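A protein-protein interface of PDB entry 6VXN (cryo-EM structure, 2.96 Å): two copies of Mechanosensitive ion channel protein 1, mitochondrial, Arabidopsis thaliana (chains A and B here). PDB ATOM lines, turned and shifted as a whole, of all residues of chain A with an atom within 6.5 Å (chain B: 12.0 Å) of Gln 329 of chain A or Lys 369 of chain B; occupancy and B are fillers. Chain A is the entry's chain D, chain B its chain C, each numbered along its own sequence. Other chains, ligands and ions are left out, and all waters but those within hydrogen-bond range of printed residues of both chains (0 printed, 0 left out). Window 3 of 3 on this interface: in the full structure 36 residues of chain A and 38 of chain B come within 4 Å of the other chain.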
ATOM      1  N   PRO A 327     -25.008  14.360  25.838  1.00  0.00           N
ATOM      2  CA  PRO A 327     -25.824  15.431  25.269  1.00  0.00           C
ATOM      3  C   PRO A 327     -25.259  15.919  23.946  1.00  0.00           C
ATOM      4  O   PRO A 327     -24.050  15.903  23.710  1.00  0.00           O
ATOM      5  CB  PRO A 327     -25.756  16.522  26.340  1.00  0.00           C
ATOM      6  CG  PRO A 327     -24.434  16.325  26.957  1.00  0.00           C
ATOM      7  CD  PRO A 327     -24.146  14.852  26.925  1.00  0.00           C
ATOM      8  N   LEU A 328     -26.160  16.351  23.073  1.00  0.00           N
ATOM      9  CA  LEU A 328     -25.834  16.711  21.703  1.00  0.00           C
ATOM     10  C   LEU A 328     -26.388  18.089  21.384  1.00  0.00           C
ATOM     11  O   LEU A 328     -27.516  18.414  21.761  1.00  0.00           O
ATOM     12  CB  LEU A 328     -26.417  15.705  20.711  1.00  0.00           C
ATOM     13  CG  LEU A 328     -25.600  14.552  20.135  1.00  0.00           C
ATOM     14  CD1 LEU A 328     -24.887  13.785  21.205  1.00  0.00           C
ATOM     15  CD2 LEU A 328     -26.514  13.630  19.362  1.00  0.00           C
ATOM     16  N   GLN A 329     -25.597  18.900  20.691  1.00  0.00           N
ATOM     17  CA  GLN A 329     -26.080  20.157  20.124  1.00  0.00           C
ATOM     18  C   GLN A 329     -26.271  19.912  18.637  1.00  0.00           C
ATOM     19  O   GLN A 329     -25.379  20.151  17.827  1.00  0.00           O
ATOM     20  CB  GLN A 329     -25.122  21.306  20.382  1.00  0.00           C
ATOM     21  CG  GLN A 329     -25.689  22.654  20.004  1.00  0.00           C
ATOM     22  CD  GLN A 329     -24.723  23.777  20.274  1.00  0.00           C
ATOM     23  OE1 GLN A 329     -25.013  24.691  21.044  1.00  0.00           O
ATOM     24  NE2 GLN A 329     -23.563  23.719  19.634  1.00  0.00           N
ATOM     25  N   ILE A 330     -27.447  19.416  18.282  1.00  0.00           N
ATOM     26  CA  ILE A 330     -27.764  19.060  16.910  1.00  0.00           C
ATOM     27  C   ILE A 330     -29.113  19.673  16.562  1.00  0.00           C
ATOM     28  O   ILE A 330     -30.061  19.602  17.353  1.00  0.00           O
ATOM     29  CB  ILE A 330     -27.738  17.529  16.710  1.00  0.00           C
ATOM     30  CG1 ILE A 330     -28.133  17.128  15.295  1.00  0.00           C
ATOM     31  CG2 ILE A 330     -28.551  16.789  17.766  1.00  0.00           C
ATOM     32  CD1 ILE A 330     -27.775  15.697  14.987  1.00  0.00           C
ATOM     33  N   ASP A 331     -29.178  20.336  15.412  1.00  0.00           N
ATOM     34  CA  ASP A 331     -30.408  20.974  14.965  1.00  0.00           C
ATOM     35  C   ASP A 331     -31.176  20.141  13.956  1.00  0.00           C
ATOM     36  O   ASP A 331     -32.400  20.267  13.874  1.00  0.00           O
ATOM     37  CB  ASP A 331     -30.106  22.340  14.346  1.00  0.00           C
ATOM     38  CG  ASP A 331     -29.981  23.429  15.383  1.00  0.00           C
ATOM     39  OD1 ASP A 331     -29.835  23.095  16.573  1.00  0.00           O
ATOM     40  OD2 ASP A 331     -30.026  24.618  15.008  1.00  0.00           O
ATOM     41  N   SER A 370     -31.931  22.766  20.066  1.00  0.00           N
ATOM     42  CA  SER A 370     -30.498  22.597  19.803  1.00  0.00           C
ATOM     43  C   SER A 370     -29.876  21.597  20.769  1.00  0.00           C
ATOM     44  O   SER A 370     -28.767  21.788  21.272  1.00  0.00           O
ATOM     45  CB  SER A 370     -29.760  23.937  19.848  1.00  0.00           C
ATOM     46  OG  SER A 370     -30.247  24.818  18.855  1.00  0.00           O
ATOM     47  N   PHE A 371     -30.611  20.525  21.046  1.00  0.00           N
ATOM     48  CA  PHE A 371     -30.240  19.621  22.119  1.00  0.00           C
ATOM     49  C   PHE A 371     -30.865  18.266  21.846  1.00  0.00           C
ATOM     50  O   PHE A 371     -31.988  18.179  21.348  1.00  0.00           O
ATOM     51  CB  PHE A 371     -30.696  20.165  23.480  1.00  0.00           C
ATOM     52  CG  PHE A 371     -30.315  19.303  24.648  1.00  0.00           C
ATOM     53  CD1 PHE A 371     -29.066  19.420  25.225  1.00  0.00           C
ATOM     54  CD2 PHE A 371     -31.213  18.399  25.189  1.00  0.00           C
ATOM     55  CE1 PHE A 371     -28.713  18.637  26.304  1.00  0.00           C
ATOM     56  CE2 PHE A 371     -30.863  17.616  26.262  1.00  0.00           C
ATOM     57  CZ  PHE A 371     -29.613  17.736  26.822  1.00  0.00           C
ATOM     58  N   ALA A 372     -30.119  17.221  22.166  1.00  0.00           N
ATOM     59  CA  ALA A 372     -30.610  15.856  22.147  1.00  0.00           C
ATOM     60  C   ALA A 372     -29.831  15.102  23.207  1.00  0.00           C
ATOM     61  O   ALA A 372     -28.837  15.597  23.732  1.00  0.00           O
ATOM     62  CB  ALA A 372     -30.449  15.221  20.765  1.00  0.00           C
ATOM     63  N   GLY A 407     -19.960  15.558  12.015  1.00  0.00           N
ATOM     64  CA  GLY A 407     -20.126  16.996  12.060  1.00  0.00           C
ATOM     65  C   GLY A 407     -21.209  17.443  13.017  1.00  0.00           C
ATOM     66  O   GLY A 407     -22.025  18.303  12.681  1.00  0.00           O
ATOM     67  N   VAL A 408     -21.232  16.858  14.213  1.00  0.00           N
ATOM     68  CA  VAL A 408     -22.211  17.179  15.247  1.00  0.00           C
ATOM     69  C   VAL A 408     -21.455  17.467  16.532  1.00  0.00           C
ATOM     70  O   VAL A 408     -20.734  16.599  17.035  1.00  0.00           O
ATOM     71  CB  VAL A 408     -23.217  16.038  15.470  1.00  0.00           C
ATOM     72  CG1 VAL A 408     -24.112  16.360  16.640  1.00  0.00           C
ATOM     73  CG2 VAL A 408     -24.053  15.796  14.229  1.00  0.00           C
ATOM     74  N   SER A 409     -21.620  18.671  17.069  1.00  0.00           N
ATOM     75  CA  SER A 409     -20.951  19.034  18.305  1.00  0.00           C
ATOM     76  C   SER A 409     -21.760  18.564  19.514  1.00  0.00           C
ATOM     77  O   SER A 409     -22.922  18.168  19.404  1.00  0.00           O
ATOM     78  CB  SER A 409     -20.726  20.544  18.367  1.00  0.00           C
ATOM     79  OG  SER A 409     -21.889  21.249  17.972  1.00  0.00           O
ATOM     80  N   LEU A 410     -21.122  18.606  20.678  1.00  0.00           N
ATOM     81  CA  LEU A 410     -21.778  18.212  21.914  1.00  0.00           C
ATOM     82  C   LEU A 410     -22.657  19.343  22.430  1.00  0.00           C
ATOM     83  O   LEU A 410     -22.442  20.516  22.126  1.00  0.00           O
ATOM     84  CB  LEU A 410     -20.747  17.828  22.972  1.00  0.00           C
ATOM     85  CG  LEU A 410     -19.894  16.598  22.675  1.00  0.00           C
ATOM     86  CD1 LEU A 410     -18.627  16.628  23.497  1.00  0.00           C
ATOM     87  CD2 LEU A 410     -20.676  15.342  22.946  1.00  0.00           C
ATOM     88  N   GLY A 411     -23.668  18.975  23.221  1.00  0.00           N
ATOM     89  CA  GLY A 411     -24.588  19.931  23.792  1.00  0.00           C
ATOM     90  C   GLY A 411     -24.298  20.202  25.258  1.00  0.00           C
ATOM     91  O   GLY A 411     -23.456  19.570  25.886  1.00  0.00           O
ATOM     92  N   THR A 412     -25.024  21.171  25.803  1.00  0.00           N
ATOM     93  CA  THR A 412     -24.818  21.601  27.175  1.00  0.00           C
ATOM     94  C   THR A 412     -26.105  21.444  27.972  1.00  0.00           C
ATOM     95  O   THR A 412     -27.207  21.624  27.444  1.00  0.00           O
ATOM     96  CB  THR A 412     -24.294  23.054  27.241  1.00  0.00           C
ATOM     97  OG1 THR A 412     -24.065  23.429  28.606  1.00  0.00           O
ATOM     98  CG2 THR A 412     -25.243  24.044  26.577  1.00  0.00           C
ATOM     99  N   PRO B 327     -12.663  18.731  36.711  1.00  0.00           N
ATOM    100  CA  PRO B 327     -13.305  19.079  35.444  1.00  0.00           C
ATOM    101  C   PRO B 327     -12.314  19.694  34.469  1.00  0.00           C
ATOM    102  O   PRO B 327     -11.354  20.361  34.853  1.00  0.00           O
ATOM    103  CB  PRO B 327     -14.372  20.091  35.865  1.00  0.00           C
ATOM    104  CG  PRO B 327     -13.786  20.748  37.045  1.00  0.00           C
ATOM    105  CD  PRO B 327     -12.961  19.718  37.760  1.00  0.00           C
ATOM    106  N   LEU B 328     -12.560  19.450  33.187  1.00  0.00           N
ATOM    107  CA  LEU B 328     -11.647  19.819  32.117  1.00  0.00           C
ATOM    108  C   LEU B 328     -12.396  20.589  31.042  1.00  0.00           C
ATOM    109  O   LEU B 328     -13.518  20.230  30.678  1.00  0.00           O
ATOM    110  CB  LEU B 328     -11.010  18.582  31.483  1.00  0.00           C
ATOM    111  CG  LEU B 328      -9.630  18.074  31.886  1.00  0.00           C
ATOM    112  CD1 LEU B 328      -9.491  17.954  33.372  1.00  0.00           C
ATOM    113  CD2 LEU B 328      -9.382  16.734  31.235  1.00  0.00           C
ATOM    114  N   GLN B 329     -11.776  21.647  30.534  1.00  0.00           N
ATOM    115  CA  GLN B 329     -12.273  22.341  29.347  1.00  0.00           C
ATOM    116  C   GLN B 329     -11.382  21.909  28.194  1.00  0.00           C
ATOM    117  O   GLN B 329     -10.386  22.553  27.875  1.00  0.00           O
ATOM    118  CB  GLN B 329     -12.267  23.849  29.522  1.00  0.00           C
ATOM    119  CG  GLN B 329     -12.975  24.582  28.407  1.00  0.00           C
ATOM    120  CD  GLN B 329     -12.961  26.075  28.606  1.00  0.00           C
ATOM    121  OE1 GLN B 329     -14.010  26.712  28.698  1.00  0.00           O
ATOM    122  NE2 GLN B 329     -11.766  26.647  28.667  1.00  0.00           N
ATOM    123  N   ILE B 330     -11.746  20.796  27.573  1.00  0.00           N
ATOM    124  CA  ILE B 330     -10.965  20.211  26.496  1.00  0.00           C
ATOM    125  C   ILE B 330     -11.909  19.899  25.344  1.00  0.00           C
ATOM    126  O   ILE B 330     -13.001  19.356  25.551  1.00  0.00           O
ATOM    127  CB  ILE B 330     -10.188  18.968  26.983  1.00  0.00           C
ATOM    128  CG1 ILE B 330      -9.415  18.298  25.855  1.00  0.00           C
ATOM    129  CG2 ILE B 330     -11.075  17.984  27.737  1.00  0.00           C
ATOM    130  CD1 ILE B 330      -8.391  17.319  26.369  1.00  0.00           C
ATOM    131  N   ASP B 331     -11.519  20.304  24.139  1.00  0.00           N
ATOM    132  CA  ASP B 331     -12.333  20.073  22.955  1.00  0.00           C
ATOM    133  C   ASP B 331     -11.880  18.870  22.150  1.00  0.00           C
ATOM    134  O   ASP B 331     -12.702  18.256  21.463  1.00  0.00           O
ATOM    135  CB  ASP B 331     -12.318  21.303  22.047  1.00  0.00           C
ATOM    136  CG  ASP B 331     -13.324  22.346  22.470  1.00  0.00           C
ATOM    137  OD1 ASP B 331     -13.821  22.257  23.608  1.00  0.00           O
ATOM    138  OD2 ASP B 331     -13.619  23.253  21.666  1.00  0.00           O
ATOM    139  N   ASP B 332     -10.601  18.520  22.219  1.00  0.00           N
ATOM    140  CA  ASP B 332     -10.043  17.389  21.491  1.00  0.00           C
ATOM    141  C   ASP B 332      -9.633  16.337  22.510  1.00  0.00           C
ATOM    142  O   ASP B 332      -8.603  16.478  23.173  1.00  0.00           O
ATOM    143  CB  ASP B 332      -8.857  17.834  20.642  1.00  0.00           C
ATOM    144  CG  ASP B 332      -8.742  17.057  19.355  1.00  0.00           C
ATOM    145  OD1 ASP B 332      -8.840  15.817  19.390  1.00  0.00           O
ATOM    146  OD2 ASP B 332      -8.556  17.687  18.297  1.00  0.00           O
ATOM    147  N   LEU B 333     -10.429  15.278  22.618  1.00  0.00           N
ATOM    148  CA  LEU B 333     -10.265  14.301  23.683  1.00  0.00           C
ATOM    149  C   LEU B 333      -9.186  13.275  23.370  1.00  0.00           C
ATOM    150  O   LEU B 333      -8.974  12.369  24.182  1.00  0.00           O
ATOM    151  CB  LEU B 333     -11.592  13.602  23.956  1.00  0.00           C
ATOM    152  CG  LEU B 333     -12.825  14.458  24.219  1.00  0.00           C
ATOM    153  CD1 LEU B 333     -13.977  13.556  24.558  1.00  0.00           C
ATOM    154  CD2 LEU B 333     -12.568  15.419  25.354  1.00  0.00           C
ATOM    155  N   ILE B 336      -6.786  12.735  26.131  1.00  0.00           N
ATOM    156  CA  ILE B 336      -7.348  12.196  27.373  1.00  0.00           C
ATOM    157  C   ILE B 336      -6.667  10.914  27.865  1.00  0.00           C
ATOM    158  O   ILE B 336      -6.421  10.826  29.077  1.00  0.00           O
ATOM    159  CB  ILE B 336      -8.875  12.022  27.225  1.00  0.00           C
ATOM    160  CG1 ILE B 336      -9.570  13.381  27.303  1.00  0.00           C
ATOM    161  CG2 ILE B 336      -9.480  11.085  28.267  1.00  0.00           C
ATOM    162  CD1 ILE B 336      -9.556  13.992  28.668  1.00  0.00           C
ATOM    163  N   LEU B 364     -12.141   8.615  32.968  1.00  0.00           N
ATOM    164  CA  LEU B 364     -13.039   9.646  32.463  1.00  0.00           C
ATOM    165  C   LEU B 364     -14.472   9.229  32.767  1.00  0.00           C
ATOM    166  O   LEU B 364     -14.952   8.218  32.246  1.00  0.00           O
ATOM    167  CB  LEU B 364     -12.833   9.839  30.965  1.00  0.00           C
ATOM    168  CG  LEU B 364     -13.807  10.755  30.241  1.00  0.00           C
ATOM    169  CD1 LEU B 364     -13.408  12.186  30.447  1.00  0.00           C
ATOM    170  CD2 LEU B 364     -13.836  10.426  28.775  1.00  0.00           C
ATOM    171  N   SER B 365     -15.151  10.001  33.610  1.00  0.00           N
ATOM    172  CA  SER B 365     -16.459   9.597  34.106  1.00  0.00           C
ATOM    173  C   SER B 365     -17.617  10.161  33.301  1.00  0.00           C
ATOM    174  O   SER B 365     -18.641   9.483  33.160  1.00  0.00           O
ATOM    175  CB  SER B 365     -16.627  10.019  35.565  1.00  0.00           C
ATOM    176  OG  SER B 365     -16.606  11.425  35.688  1.00  0.00           O
ATOM    177  N   ARG B 366     -17.488  11.370  32.767  1.00  0.00           N
ATOM    178  CA  ARG B 366     -18.573  11.969  32.005  1.00  0.00           C
ATOM    179  C   ARG B 366     -18.003  13.011  31.061  1.00  0.00           C
ATOM    180  O   ARG B 366     -16.931  13.569  31.296  1.00  0.00           O
ATOM    181  CB  ARG B 366     -19.641  12.586  32.909  1.00  0.00           C
ATOM    182  CG  ARG B 366     -19.158  13.733  33.760  1.00  0.00           C
ATOM    183  CD  ARG B 366     -20.257  14.176  34.696  1.00  0.00           C
ATOM    184  NE  ARG B 366     -21.457  14.542  33.959  1.00  0.00           N
ATOM    185  CZ  ARG B 366     -21.795  15.789  33.656  1.00  0.00           C
ATOM    186  NH1 ARG B 366     -22.906  16.030  32.977  1.00  0.00           N
ATOM    187  NH2 ARG B 366     -21.034  16.795  34.055  1.00  0.00           N
ATOM    188  N   VAL B 367     -18.745  13.269  29.984  1.00  0.00           N
ATOM    189  CA  VAL B 367     -18.310  14.179  28.935  1.00  0.00           C
ATOM    190  C   VAL B 367     -19.479  15.105  28.613  1.00  0.00           C
ATOM    191  O   VAL B 367     -20.636  14.805  28.914  1.00  0.00           O
ATOM    192  CB  VAL B 367     -17.821  13.399  27.686  1.00  0.00           C
ATOM    193  CG1 VAL B 367     -18.984  12.820  26.897  1.00  0.00           C
ATOM    194  CG2 VAL B 367     -16.868  14.216  26.821  1.00  0.00           C
ATOM    195  N   GLU B 368     -19.159  16.250  28.009  1.00  0.00           N
ATOM    196  CA  GLU B 368     -20.104  17.323  27.708  1.00  0.00           C
ATOM    197  C   GLU B 368     -19.394  18.279  26.751  1.00  0.00           C
ATOM    198  O   GLU B 368     -18.223  18.076  26.416  1.00  0.00           O
ATOM    199  CB  GLU B 368     -20.560  18.013  28.996  1.00  0.00           C
ATOM    200  CG  GLU B 368     -21.941  18.608  28.956  1.00  0.00           C
ATOM    201  CD  GLU B 368     -22.512  18.824  30.329  1.00  0.00           C
ATOM    202  OE1 GLU B 368     -22.484  17.871  31.133  1.00  0.00           O
ATOM    203  OE2 GLU B 368     -22.979  19.946  30.607  1.00  0.00           O
ATOM    204  N   LYS B 369     -20.107  19.316  26.299  1.00  0.00           N
ATOM    205  CA  LYS B 369     -19.532  20.297  25.376  1.00  0.00           C
ATOM    206  C   LYS B 369     -18.454  21.117  26.065  1.00  0.00           C
ATOM    207  O   LYS B 369     -18.737  21.799  27.058  1.00  0.00           O
ATOM    208  CB  LYS B 369     -20.597  21.240  24.833  1.00  0.00           C
ATOM    209  CG  LYS B 369     -20.042  22.220  23.820  1.00  0.00           C
ATOM    210  CD  LYS B 369     -21.029  23.306  23.457  1.00  0.00           C
ATOM    211  CE  LYS B 369     -20.635  23.962  22.146  1.00  0.00           C
ATOM    212  NZ  LYS B 369     -21.588  25.031  21.738  1.00  0.00           N
ATOM    213  N   SER B 370     -17.238  21.064  25.506  1.00  0.00           N
ATOM    214  CA  SER B 370     -16.046  21.733  26.036  1.00  0.00           C
ATOM    215  C   SER B 370     -15.810  21.364  27.495  1.00  0.00           C
ATOM    216  O   SER B 370     -15.456  22.201  28.326  1.00  0.00           O
ATOM    217  CB  SER B 370     -16.138  23.252  25.864  1.00  0.00           C
ATOM    218  OG  SER B 370     -16.218  23.603  24.495  1.00  0.00           O
ATOM    219  N   PHE B 371     -16.027  20.090  27.810  1.00  0.00           N
ATOM    220  CA  PHE B 371     -16.063  19.660  29.196  1.00  0.00           C
ATOM    221  C   PHE B 371     -15.751  18.177  29.248  1.00  0.00           C
ATOM    222  O   PHE B 371     -16.160  17.416  28.371  1.00  0.00           O
ATOM    223  CB  PHE B 371     -17.433  19.949  29.826  1.00  0.00           C
ATOM    224  CG  PHE B 371     -17.538  19.566  31.275  1.00  0.00           C
ATOM    225  CD1 PHE B 371     -17.106  20.434  32.260  1.00  0.00           C
ATOM    226  CD2 PHE B 371     -18.098  18.359  31.652  1.00  0.00           C
ATOM    227  CE1 PHE B 371     -17.209  20.091  33.592  1.00  0.00           C
ATOM    228  CE2 PHE B 371     -18.197  18.014  32.978  1.00  0.00           C
ATOM    229  CZ  PHE B 371     -17.756  18.881  33.948  1.00  0.00           C
ATOM    230  N   ALA B 372     -15.013  17.788  30.277  1.00  0.00           N
ATOM    231  CA  ALA B 372     -14.764  16.395  30.595  1.00  0.00           C
ATOM    232  C   ALA B 372     -14.581  16.321  32.098  1.00  0.00           C
ATOM    233  O   ALA B 372     -14.444  17.342  32.769  1.00  0.00           O
ATOM    234  CB  ALA B 372     -13.541  15.861  29.849  1.00  0.00           C
ATOM    235  N   GLU B 373     -14.569  15.112  32.637  1.00  0.00           N
ATOM    236  CA  GLU B 373     -14.368  14.971  34.069  1.00  0.00           C
ATOM    237  C   GLU B 373     -13.501  13.761  34.344  1.00  0.00           C
ATOM    238  O   GLU B 373     -13.807  12.659  33.883  1.00  0.00           O
ATOM    239  CB  GLU B 373     -15.697  14.844  34.803  1.00  0.00           C
ATOM    240  CG  GLU B 373     -15.546  14.807  36.296  1.00  0.00           C
ATOM    241  CD  GLU B 373     -16.858  14.988  37.008  1.00  0.00           C
ATOM    242  OE1 GLU B 373     -17.731  14.105  36.881  1.00  0.00           O
ATOM    243  OE2 GLU B 373     -17.022  16.018  37.693  1.00  0.00           O
ATOM    244  N   VAL B 408      -4.016  21.987  28.328  1.00  0.00           N
ATOM    245  CA  VAL B 408      -5.442  21.765  28.551  1.00  0.00           C
ATOM    246  C   VAL B 408      -5.847  22.543  29.792  1.00  0.00           C
ATOM    247  O   VAL B 408      -5.314  22.297  30.879  1.00  0.00           O
ATOM    248  CB  VAL B 408      -5.779  20.275  28.727  1.00  0.00           C
ATOM    249  CG1 VAL B 408      -7.233  20.115  29.095  1.00  0.00           C
ATOM    250  CG2 VAL B 408      -5.473  19.494  27.466  1.00  0.00           C
ATOM    251  N   SER B 409      -6.788  23.467  29.639  1.00  0.00           N
ATOM    252  CA  SER B 409      -7.253  24.252  30.771  1.00  0.00           C
ATOM    253  C   SER B 409      -8.343  23.500  31.534  1.00  0.00           C
ATOM    254  O   SER B 409      -8.889  22.498  31.071  1.00  0.00           O
ATOM    255  CB  SER B 409      -7.768  25.611  30.302  1.00  0.00           C
ATOM    256  OG  SER B 409      -8.596  25.477  29.161  1.00  0.00           O
ATOM    257  N   LEU B 410      -8.651  23.999  32.726  1.00  0.00           N
ATOM    258  CA  LEU B 410      -9.687  23.402  33.553  1.00  0.00           C
ATOM    259  C   LEU B 410     -11.063  23.853  33.081  1.00  0.00           C
ATOM    260  O   LEU B 410     -11.219  24.904  32.460  1.00  0.00           O
ATOM    261  CB  LEU B 410      -9.489  23.776  35.019  1.00  0.00           C
ATOM    262  CG  LEU B 410      -8.223  23.247  35.690  1.00  0.00           C
ATOM    263  CD1 LEU B 410      -7.894  24.073  36.911  1.00  0.00           C
ATOM    264  CD2 LEU B 410      -8.392  21.797  36.056  1.00  0.00           C
ATOM    265  N   GLY B 411     -12.074  23.034  33.382  1.00  0.00           N
ATOM    266  CA  GLY B 411     -13.439  23.323  33.009  1.00  0.00           C
ATOM    267  C   GLY B 411     -14.259  23.831  34.181  1.00  0.00           C
ATOM    268  O   GLY B 411     -13.821  23.859  35.325  1.00  0.00           O
ATOM    269  N   THR B 412     -15.483  24.242  33.871  1.00  0.00           N
ATOM    270  CA  THR B 412     -16.370  24.823  34.865  1.00  0.00           C
ATOM    271  C   THR B 412     -17.657  24.015  34.955  1.00  0.00           C
ATOM    272  O   THR B 412     -18.145  23.480  33.955  1.00  0.00           O
ATOM    273  CB  THR B 412     -16.663  26.310  34.563  1.00  0.00           C
ATOM    274  OG1 THR B 412     -17.506  26.858  35.584  1.00  0.00           O
ATOM    275  CG2 THR B 412     -17.303  26.508  33.193  1.00  0.00           C
ATOM    276  N   THR B 413     -18.175  23.893  36.173  1.00  0.00           N
ATOM    277  CA  THR B 413     -19.378  23.123  36.457  1.00  0.00           C
ATOM    278  C   THR B 413     -20.470  24.083  36.900  1.00  0.00           C
ATOM    279  O   THR B 413     -20.235  24.922  37.779  1.00  0.00           O
ATOM    280  CB  THR B 413     -19.112  22.075  37.536  1.00  0.00           C
ATOM    281  OG1 THR B 413     -17.826  21.484  37.319  1.00  0.00           O
ATOM    282  CG2 THR B 413     -20.168  20.987  37.488  1.00  0.00           C
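NE2 of Gln 329 of chain A sits close to NZ of Lys 369 of chain B (3.2 Å). The backbone carbonyl oxygen of Gly 411 of chain A is in hydrogen-bond range of the backbone NH of Lys 369 of chain B, at 3.4 Å.
Gln 329 of chain A touches just one residue of chain B: Lys 369. Of chain A, only Gln 329, Leu 410 and Gly 411 come within 4 Å of Lys 369 of chain B. Pro 327 of chain A touches just one residue of chain B: Glu 368 (3.9 Å). No residue of chain B comes within 4 Å of Ile 330 of chain A. No residue of chain B comes within 4 Å of Asp 331 of chain A. No residue of chain B comes within 4 Å of Ser 370 of chain A. No residue of chain B comes within 4 Å of Phe 371 of chain A. No residue of chain B comes within 4 Å of Ala 372 of chain A. Printed residues of chain B within 4 Å of Leu 410 of chain A: Glu 368 (3.3 Å) and Lys 369 (3.4 Å). Gly 411 of chain A touches two residues of chain B. No residue of chain B comes within 4 Å of Thr 412 of chain A. Printed residues of chain A within 4 Å of Glu 368 of chain B: Pro 327 (3.9 Å), Leu 410 (3.3 Å) and Gly 411 (3.6 Å). The nearest residue of chain B that does not touch Gln 329 of chain A is Glu 368 of chain B (8.7 Å). The nearest residue of chain A that does not touch Lys 369 of chain B is Thr 412 of chain A (4.5 Å). The nearest printed residue of chain A that does not touch Glu 368 of chain B is Thr 412 of chain A (4.2 Å).
The guanidinium group (NH1) of Arg 366 of chain B is in salt-bridge range of the side-chain carboxylate (OE1) of Glu 368 of chain B, at 2.6 Å. O of Pro 327 of chain A sits at hydrogen-bond distance from N of Gly 411 of chain A (3.1 Å). The backbone NH (N) of Gln 329 of chain A lies within hydrogen-bond range of the backbone carbonyl oxygen (O) of Ser 409 of chain A (3.1 Å).
Positions printed for both chains: 327, 328, 329, 330, 331, 370, 371, 372, 408, 409, 410, 411 and 412. Of the 6 pairs that touch across the chains among the printed residues, none has its exchanged pair printed and touching as well.
Hydrophobic or aromatic side chains of chain A that line the printed part of chain B: Pro 327 and Leu 410. Of the 24 printed residues of chain B, 2 touch a printed residue of chain A.
CG of Pro 327 of chain A touches CG of Glu 368 of chain B, 3.9 Å away. O of Glu 368 of chain B touches CD1 of Leu 410 of chain A (3.3 Å). Lys 369 of chain B touches Leu 410 of chain A. CG of Glu 368 of chain B touches O of Gly 411 of chain A, 3.6 Å away.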
